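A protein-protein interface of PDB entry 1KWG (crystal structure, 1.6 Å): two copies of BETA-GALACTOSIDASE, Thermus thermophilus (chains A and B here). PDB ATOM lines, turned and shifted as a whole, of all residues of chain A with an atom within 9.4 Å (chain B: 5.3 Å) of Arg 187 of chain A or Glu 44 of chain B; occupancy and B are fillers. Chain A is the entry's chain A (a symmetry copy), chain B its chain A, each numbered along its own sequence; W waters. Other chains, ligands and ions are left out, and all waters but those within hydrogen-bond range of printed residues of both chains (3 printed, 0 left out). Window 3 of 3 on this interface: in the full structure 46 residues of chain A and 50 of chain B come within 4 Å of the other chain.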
ATOM      1  N   GLU A 164       7.461  17.564  -6.589  1.00  0.00           N
ATOM      2  CA  GLU A 164       8.162  17.299  -7.834  1.00  0.00           C
ATOM      3  C   GLU A 164       9.589  16.842  -7.547  1.00  0.00           C
ATOM      4  O   GLU A 164      10.121  15.976  -8.240  1.00  0.00           O
ATOM      5  CB  GLU A 164       8.159  18.546  -8.722  1.00  0.00           C
ATOM      6  CG  GLU A 164       8.801  18.328 -10.082  1.00  0.00           C
ATOM      7  CD  GLU A 164       8.318  19.323 -11.119  1.00  0.00           C
ATOM      8  OE1 GLU A 164       8.326  20.538 -10.829  1.00  0.00           O
ATOM      9  OE2 GLU A 164       7.934  18.889 -12.226  1.00  0.00           O
ATOM     10  N   THR A 169       8.158  12.720 -11.301  1.00  0.00           N
ATOM     11  CA  THR A 169       7.054  12.824 -12.250  1.00  0.00           C
ATOM     12  C   THR A 169       5.716  12.659 -11.541  1.00  0.00           C
ATOM     13  O   THR A 169       5.631  12.011 -10.494  1.00  0.00           O
ATOM     14  CB  THR A 169       7.142  11.739 -13.339  1.00  0.00           C
ATOM     15  OG1 THR A 169       6.979  10.447 -12.740  1.00  0.00           O
ATOM     16  CG2 THR A 169       8.490  11.801 -14.045  1.00  0.00           C
ATOM     17  N   ILE A 170       4.671  13.241 -12.114  1.00  0.00           N
ATOM     18  CA  ILE A 170       3.346  13.140 -11.522  1.00  0.00           C
ATOM     19  C   ILE A 170       2.884  11.683 -11.584  1.00  0.00           C
ATOM     20  O   ILE A 170       2.089  11.239 -10.752  1.00  0.00           O
ATOM     21  CB  ILE A 170       2.339  14.063 -12.250  1.00  0.00           C
ATOM     22  CG1 ILE A 170       1.047  14.169 -11.434  1.00  0.00           C
ATOM     23  CG2 ILE A 170       2.063  13.541 -13.653  1.00  0.00           C
ATOM     24  CD1 ILE A 170       1.233  14.831 -10.078  1.00  0.00           C
ATOM     25  N   GLU A 171       3.390  10.936 -12.564  1.00  0.00           N
ATOM     26  CA  GLU A 171       3.041   9.523 -12.700  1.00  0.00           C
ATOM     27  C   GLU A 171       3.472   8.776 -11.438  1.00  0.00           C
ATOM     28  O   GLU A 171       2.729   7.944 -10.909  1.00  0.00           O
ATOM     29  CB  GLU A 171       3.750   8.895 -13.908  1.00  0.00           C
ATOM     30  CG  GLU A 171       3.179   9.240 -15.281  1.00  0.00           C
ATOM     31  CD  GLU A 171       3.325  10.707 -15.646  1.00  0.00           C
ATOM     32  OE1 GLU A 171       4.393  11.291 -15.368  1.00  0.00           O
ATOM     33  OE2 GLU A 171       2.373  11.271 -16.227  1.00  0.00           O
ATOM     34  N   LEU A 173       3.905  10.051  -8.494  1.00  0.00           N
ATOM     35  CA  LEU A 173       3.088  10.488  -7.366  1.00  0.00           C
ATOM     36  C   LEU A 173       1.749   9.753  -7.391  1.00  0.00           C
ATOM     37  O   LEU A 173       1.280   9.263  -6.361  1.00  0.00           O
ATOM     38  CB  LEU A 173       2.865  12.008  -7.410  1.00  0.00           C
ATOM     39  CG  LEU A 173       1.975  12.618  -6.310  1.00  0.00           C
ATOM     40  CD1 LEU A 173       2.334  14.078  -6.106  1.00  0.00           C
ATOM     41  CD2 LEU A 173       0.502  12.482  -6.680  1.00  0.00           C
ATOM     42  N   ASN A 174       1.131   9.671  -8.567  1.00  0.00           N
ATOM     43  CA  ASN A 174      -0.152   8.982  -8.684  1.00  0.00           C
ATOM     44  C   ASN A 174      -0.053   7.533  -8.223  1.00  0.00           C
ATOM     45  O   ASN A 174      -0.974   7.009  -7.592  1.00  0.00           O
ATOM     46  CB  ASN A 174      -0.670   9.023 -10.126  1.00  0.00           C
ATOM     47  CG  ASN A 174      -1.246  10.375 -10.498  1.00  0.00           C
ATOM     48  OD1 ASN A 174      -1.933  11.009  -9.697  1.00  0.00           O
ATOM     49  ND2 ASN A 174      -0.983  10.815 -11.726  1.00  0.00           N
ATOM     50  N   THR A 179      -3.822   7.177  -6.460  1.00  0.00           N
ATOM     51  CA  THR A 179      -4.871   8.108  -6.862  1.00  0.00           C
ATOM     52  C   THR A 179      -5.987   7.587  -7.760  1.00  0.00           C
ATOM     53  O   THR A 179      -6.898   8.332  -8.108  1.00  0.00           O
ATOM     54  CB  THR A 179      -4.262   9.370  -7.496  1.00  0.00           C
ATOM     55  OG1 THR A 179      -3.464   9.003  -8.628  1.00  0.00           O
ATOM     56  CG2 THR A 179      -3.397  10.100  -6.475  1.00  0.00           C
ATOM     57  N   SER A 183     -11.055   8.521  -7.836  1.00  0.00           N
ATOM     58  CA  SER A 183     -10.702   9.400  -8.953  1.00  0.00           C
ATOM     59  C   SER A 183      -9.885  10.625  -8.562  1.00  0.00           C
ATOM     60  O   SER A 183     -10.166  11.741  -9.006  1.00  0.00           O
ATOM     61  CB  SER A 183     -11.968   9.852  -9.692  1.00  0.00           C
ATOM     62  OG  SER A 183     -12.386   8.879 -10.634  1.00  0.00           O
ATOM     63  N   GLN A 184      -8.857  10.407  -7.748  1.00  0.00           N
ATOM     64  CA  GLN A 184      -7.981  11.485  -7.301  1.00  0.00           C
ATOM     65  C   GLN A 184      -6.872  11.809  -8.304  1.00  0.00           C
ATOM     66  O   GLN A 184      -6.129  12.766  -8.108  1.00  0.00           O
ATOM     67  CB  GLN A 184      -7.329  11.110  -5.967  1.00  0.00           C
ATOM     68  CG  GLN A 184      -8.277  11.083  -4.780  1.00  0.00           C
ATOM     69  CD  GLN A 184      -7.640  10.460  -3.548  1.00  0.00           C
ATOM     70  OE1 GLN A 184      -6.562  10.868  -3.116  1.00  0.00           O
ATOM     71  NE2 GLN A 184      -8.308   9.467  -2.977  1.00  0.00           N
ATOM     72  N   ARG A 185      -6.771  11.019  -9.370  1.00  0.00           N
ATOM     73  CA  ARG A 185      -5.722  11.191 -10.379  1.00  0.00           C
ATOM     74  C   ARG A 185      -5.388  12.629 -10.769  1.00  0.00           C
ATOM     75  O   ARG A 185      -6.271  13.421 -11.098  1.00  0.00           O
ATOM     76  CB  ARG A 185      -6.067  10.396 -11.643  1.00  0.00           C
ATOM     77  CG  ARG A 185      -4.956  10.390 -12.690  1.00  0.00           C
ATOM     78  CD  ARG A 185      -5.325   9.526 -13.892  1.00  0.00           C
ATOM     79  NE  ARG A 185      -4.219   9.385 -14.838  1.00  0.00           N
ATOM     80  CZ  ARG A 185      -3.695  10.383 -15.543  1.00  0.00           C
ATOM     81  NH1 ARG A 185      -4.170  11.617 -15.422  1.00  0.00           N
ATOM     82  NH2 ARG A 185      -2.690  10.148 -16.377  1.00  0.00           N
ATOM     83  N   TYR A 186      -4.095  12.943 -10.747  1.00  0.00           N
ATOM     84  CA  TYR A 186      -3.601  14.270 -11.101  1.00  0.00           C
ATOM     85  C   TYR A 186      -2.900  14.234 -12.453  1.00  0.00           C
ATOM     86  O   TYR A 186      -2.183  13.282 -12.761  1.00  0.00           O
ATOM     87  CB  TYR A 186      -2.614  14.758 -10.038  1.00  0.00           C
ATOM     88  CG  TYR A 186      -3.236  14.905  -8.671  1.00  0.00           C
ATOM     89  CD1 TYR A 186      -4.102  15.959  -8.391  1.00  0.00           C
ATOM     90  CD2 TYR A 186      -2.998  13.961  -7.673  1.00  0.00           C
ATOM     91  CE1 TYR A 186      -4.723  16.073  -7.152  1.00  0.00           C
ATOM     92  CE2 TYR A 186      -3.615  14.066  -6.427  1.00  0.00           C
ATOM     93  CZ  TYR A 186      -4.478  15.122  -6.178  1.00  0.00           C
ATOM     94  OH  TYR A 186      -5.118  15.226  -4.964  1.00  0.00           O
ATOM     95  N   ARG A 187      -3.109  15.270 -13.259  1.00  0.00           N
ATOM     96  CA  ARG A 187      -2.470  15.350 -14.570  1.00  0.00           C
ATOM     97  C   ARG A 187      -1.098  16.001 -14.446  1.00  0.00           C
ATOM     98  O   ARG A 187      -0.245  15.833 -15.312  1.00  0.00           O
ATOM     99  CB  ARG A 187      -3.312  16.177 -15.547  1.00  0.00           C
ATOM    100  CG  ARG A 187      -4.670  15.597 -15.898  1.00  0.00           C
ATOM    101  CD  ARG A 187      -5.307  16.424 -17.007  1.00  0.00           C
ATOM    102  NE  ARG A 187      -5.462  17.824 -16.618  1.00  0.00           N
ATOM    103  CZ  ARG A 187      -5.547  18.833 -17.479  1.00  0.00           C
ATOM    104  NH1 ARG A 187      -5.490  18.604 -18.785  1.00  0.00           N
ATOM    105  NH2 ARG A 187      -5.694  20.074 -17.032  1.00  0.00           N
ATOM    106  N   SER A 188      -0.896  16.749 -13.364  1.00  0.00           N
ATOM    107  CA  SER A 188       0.370  17.437 -13.133  1.00  0.00           C
ATOM    108  C   SER A 188       0.474  17.862 -11.672  1.00  0.00           C
ATOM    109  O   SER A 188      -0.509  17.812 -10.937  1.00  0.00           O
ATOM    110  CB  SER A 188       0.448  18.684 -14.013  1.00  0.00           C
ATOM    111  OG  SER A 188      -0.517  19.637 -13.602  1.00  0.00           O
ATOM    112  N   PHE A 189       1.664  18.286 -11.256  1.00  0.00           N
ATOM    113  CA  PHE A 189       1.853  18.736  -9.883  1.00  0.00           C
ATOM    114  C   PHE A 189       1.027  20.000  -9.644  1.00  0.00           C
ATOM    115  O   PHE A 189       0.642  20.301  -8.514  1.00  0.00           O
ATOM    116  CB  PHE A 189       3.337  19.007  -9.616  1.00  0.00           C
ATOM    117  CG  PHE A 189       4.184  17.766  -9.596  1.00  0.00           C
ATOM    118  CD1 PHE A 189       4.122  16.880  -8.522  1.00  0.00           C
ATOM    119  CD2 PHE A 189       5.030  17.465 -10.659  1.00  0.00           C
ATOM    120  CE1 PHE A 189       4.889  15.715  -8.506  1.00  0.00           C
ATOM    121  CE2 PHE A 189       5.798  16.305 -10.655  1.00  0.00           C
ATOM    122  CZ  PHE A 189       5.728  15.427  -9.575  1.00  0.00           C
ATOM    123  N   ALA A 190       0.739  20.729 -10.719  1.00  0.00           N
ATOM    124  CA  ALA A 190      -0.039  21.959 -10.619  1.00  0.00           C
ATOM    125  C   ALA A 190      -1.475  21.699 -10.167  1.00  0.00           C
ATOM    126  O   ALA A 190      -2.146  22.604  -9.673  1.00  0.00           O
ATOM    127  CB  ALA A 190      -0.039  22.689 -11.963  1.00  0.00           C
ATOM    128  N   GLU A 191      -1.943  20.466 -10.342  1.00  0.00           N
ATOM    129  CA  GLU A 191      -3.301  20.114  -9.939  1.00  0.00           C
ATOM    130  C   GLU A 191      -3.392  19.682  -8.480  1.00  0.00           C
ATOM    131  O   GLU A 191      -4.487  19.553  -7.941  1.00  0.00           O
ATOM    132  CB  GLU A 191      -3.865  18.993 -10.823  1.00  0.00           C
ATOM    133  CG  GLU A 191      -4.108  19.385 -12.276  1.00  0.00           C
ATOM    134  CD  GLU A 191      -4.989  18.387 -13.013  1.00  0.00           C
ATOM    135  OE1 GLU A 191      -4.981  17.191 -12.651  1.00  0.00           O
ATOM    136  OE2 GLU A 191      -5.684  18.795 -13.969  1.00  0.00           O
ATOM    137  N   VAL A 192      -2.247  19.455  -7.844  1.00  0.00           N
ATOM    138  CA  VAL A 192      -2.246  19.033  -6.445  1.00  0.00           C
ATOM    139  C   VAL A 192      -2.418  20.218  -5.501  1.00  0.00           C
ATOM    140  O   VAL A 192      -1.752  21.248  -5.643  1.00  0.00           O
ATOM    141  CB  VAL A 192      -0.933  18.298  -6.078  1.00  0.00           C
ATOM    142  CG1 VAL A 192      -0.980  17.832  -4.622  1.00  0.00           C
ATOM    143  CG2 VAL A 192      -0.722  17.111  -7.004  1.00  0.00           C
ATOM    144  N   GLU B  42     -11.887   9.367 -18.267  1.00  0.00           N
ATOM    145  CA  GLU B  42     -11.578  10.627 -18.929  1.00  0.00           C
ATOM    146  C   GLU B  42     -10.421  11.309 -18.199  1.00  0.00           C
ATOM    147  O   GLU B  42     -10.602  12.338 -17.549  1.00  0.00           O
ATOM    148  CB  GLU B  42     -12.820  11.530 -18.949  1.00  0.00           C
ATOM    149  CG  GLU B  42     -12.634  12.846 -19.704  1.00  0.00           C
ATOM    150  CD  GLU B  42     -13.939  13.593 -19.939  1.00  0.00           C
ATOM    151  OE1 GLU B  42     -14.908  13.381 -19.181  1.00  0.00           O
ATOM    152  OE2 GLU B  42     -13.994  14.413 -20.882  1.00  0.00           O
ATOM    153  N   PRO B  43      -9.210  10.734 -18.299  1.00  0.00           N
ATOM    154  CA  PRO B  43      -8.016  11.281 -17.647  1.00  0.00           C
ATOM    155  C   PRO B  43      -7.653  12.663 -18.181  1.00  0.00           C
ATOM    156  O   PRO B  43      -7.129  13.507 -17.452  1.00  0.00           O
ATOM    157  CB  PRO B  43      -6.951  10.230 -17.946  1.00  0.00           C
ATOM    158  CG  PRO B  43      -7.376   9.700 -19.275  1.00  0.00           C
ATOM    159  CD  PRO B  43      -8.868   9.551 -19.108  1.00  0.00           C
ATOM    160  N   GLU B  44      -7.932  12.875 -19.463  1.00  0.00           N
ATOM    161  CA  GLU B  44      -7.684  14.151 -20.124  1.00  0.00           C
ATOM    162  C   GLU B  44      -9.039  14.666 -20.598  1.00  0.00           C
ATOM    163  O   GLU B  44      -9.855  13.900 -21.107  1.00  0.00           O
ATOM    164  CB  GLU B  44      -6.758  13.970 -21.332  1.00  0.00           C
ATOM    165  CG  GLU B  44      -5.284  13.771 -21.003  1.00  0.00           C
ATOM    166  CD  GLU B  44      -4.674  14.963 -20.287  1.00  0.00           C
ATOM    167  OE1 GLU B  44      -5.118  16.104 -20.534  1.00  0.00           O
ATOM    168  OE2 GLU B  44      -3.736  14.761 -19.487  1.00  0.00           O
ATOM    169  N   PRO B  45      -9.299  15.972 -20.435  1.00  0.00           N
ATOM    170  CA  PRO B  45     -10.575  16.556 -20.857  1.00  0.00           C
ATOM    171  C   PRO B  45     -10.949  16.216 -22.301  1.00  0.00           C
ATOM    172  O   PRO B  45     -10.186  16.494 -23.228  1.00  0.00           O
ATOM    173  CB  PRO B  45     -10.345  18.053 -20.671  1.00  0.00           C
ATOM    174  CG  PRO B  45      -9.367  18.108 -19.539  1.00  0.00           C
ATOM    175  CD  PRO B  45      -8.404  17.003 -19.881  1.00  0.00           C
ATOM    176  N   GLY B  46     -12.117  15.608 -22.484  1.00  0.00           N
ATOM    177  CA  GLY B  46     -12.573  15.268 -23.821  1.00  0.00           C
ATOM    178  C   GLY B  46     -11.976  14.019 -24.439  1.00  0.00           C
ATOM    179  O   GLY B  46     -12.396  13.600 -25.518  1.00  0.00           O
ATOM    180  N   ARG B  47     -10.995  13.423 -23.770  1.00  0.00           N
ATOM    181  CA  ARG B  47     -10.361  12.213 -24.278  1.00  0.00           C
ATOM    182  C   ARG B  47     -10.796  11.008 -23.454  1.00  0.00           C
ATOM    183  O   ARG B  47     -10.269  10.762 -22.370  1.00  0.00           O
ATOM    184  CB  ARG B  47      -8.837  12.350 -24.234  1.00  0.00           C
ATOM    185  CG  ARG B  47      -8.284  13.448 -25.136  1.00  0.00           C
ATOM    186  CD  ARG B  47      -8.680  13.223 -26.591  1.00  0.00           C
ATOM    187  NE  ARG B  47      -8.166  14.265 -27.478  1.00  0.00           N
ATOM    188  CZ  ARG B  47      -6.878  14.444 -27.760  1.00  0.00           C
ATOM    189  NH1 ARG B  47      -5.960  13.648 -27.226  1.00  0.00           N
ATOM    190  NH2 ARG B  47      -6.508  15.420 -28.576  1.00  0.00           N
ATOM    191  N   LEU B  48     -11.766  10.263 -23.976  1.00  0.00           N
ATOM    192  CA  LEU B  48     -12.277   9.088 -23.286  1.00  0.00           C
ATOM    193  C   LEU B  48     -11.435   7.847 -23.543  1.00  0.00           C
ATOM    194  O   LEU B  48     -10.967   7.615 -24.658  1.00  0.00           O
ATOM    195  CB  LEU B  48     -13.728   8.814 -23.696  1.00  0.00           C
ATOM    196  CG  LEU B  48     -14.816   9.735 -23.134  1.00  0.00           C
ATOM    197  CD1 LEU B  48     -14.837   9.624 -21.618  1.00  0.00           C
ATOM    198  CD2 LEU B  48     -14.565  11.171 -23.560  1.00  0.00           C
ATOM    199  N   TRP B  79      -9.243  17.852 -12.977  1.00  0.00           N
ATOM    200  CA  TRP B  79      -9.231  18.792 -14.095  1.00  0.00           C
ATOM    201  C   TRP B  79     -10.598  19.435 -14.289  1.00  0.00           C
ATOM    202  O   TRP B  79     -10.694  20.576 -14.750  1.00  0.00           O
ATOM    203  CB  TRP B  79      -8.780  18.119 -15.404  1.00  0.00           C
ATOM    204  CG  TRP B  79      -9.651  16.998 -15.904  1.00  0.00           C
ATOM    205  CD1 TRP B  79      -9.394  15.658 -15.809  1.00  0.00           C
ATOM    206  CD2 TRP B  79     -10.903  17.117 -16.596  1.00  0.00           C
ATOM    207  NE1 TRP B  79     -10.405  14.938 -16.398  1.00  0.00           N
ATOM    208  CE2 TRP B  79     -11.345  15.806 -16.890  1.00  0.00           C
ATOM    209  CE3 TRP B  79     -11.696  18.202 -16.998  1.00  0.00           C
ATOM    210  CZ2 TRP B  79     -12.544  15.550 -17.565  1.00  0.00           C
ATOM    211  CZ3 TRP B  79     -12.893  17.946 -17.672  1.00  0.00           C
ATOM    212  CH2 TRP B  79     -13.302  16.630 -17.947  1.00  0.00           C
HETATM  213  O   HOH W   1      -6.561  12.792 -14.735  1.00  0.00           O
HETATM  214  O   HOH W   2      -7.087  15.433 -13.167  1.00  0.00           O
HETATM  215  O   HOH W   3      -2.842  12.951 -17.869  1.00  0.00           O
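Of chain B, only Pro 43, Glu 44, Pro 45 and Trp 79 come within 4 Å of Arg 187 of chain A.
Printed residues of chain B within 4 Å of Glu 191 of chain A: Trp 79 (3.5 Å).
Printed residues of chain A within 4 Å of Pro 43 of chain B: Arg 187 (3.5 Å).
Of chain A, only Arg 187 comes within 4 Å of Pro 45 of chain B.
No residue of chain A comes within 4 Å of Gly 46 of chain B.
Of the printed residues of chain A, Trp 79 of chain B touches Arg 187 (3.5 Å) and Glu 191 (3.5 Å).
The nearest printed residue of chain B that does not touch Arg 187 of chain A is Glu 42 of chain B (6.7 Å).
The nearest residue of chain A that does not touch Glu 44 of chain B is Arg 185 of chain A (5.2 Å).
O of Glu 42 of chain B sits at hydrogen-bond distance from NE1 of Trp 79 of chain B (2.9 Å).
NE of Arg 187 of chain A lies within salt-bridge range of OE2 of Glu 191 of chain A (2.8 Å).
No position is printed for both chains.
OE1 of Glu 44 of chain B is in salt-bridge range of NH1 of Arg 187 of chain A (3.1 Å).
Among the printed residues, merely in contact across the chains: Arg 187 of chain A with Pro 43 of chain B, Arg 187 of chain A with Pro 45 of chain B, Arg 187 of chain A with Trp 79 of chain B and Glu 191 of chain A with Trp 79 of chain B.
Of the 17 printed residues of chain A, 2 touch a printed residue of chain B.
Among the printed residues, Asp or Glu carboxylates within 4 Å of a Lys or Arg side-chain nitrogen of the other chain: Arg 187 of chain A with Glu 44 of chain B.
Water W3 lies within hydrogen-bond range of OE2 of Glu 44 of chain B and NH1 of Arg 185 of chain A.
Water W1 lies within hydrogen-bond range of the guanidinium group of Arg 185 of chain A (2.8 Å) and the backbone carbonyl oxygen of Pro 43 of chain B (2.9 Å).
Water W2 lies within hydrogen-bond range of the side-chain carboxylate of Glu 191 of chain A (2.8 Å), the backbone carbonyl oxygen of Arg 185 of chain A (3.0 Å) and the backbone NH of Trp 79 of chain B (3.2 Å).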
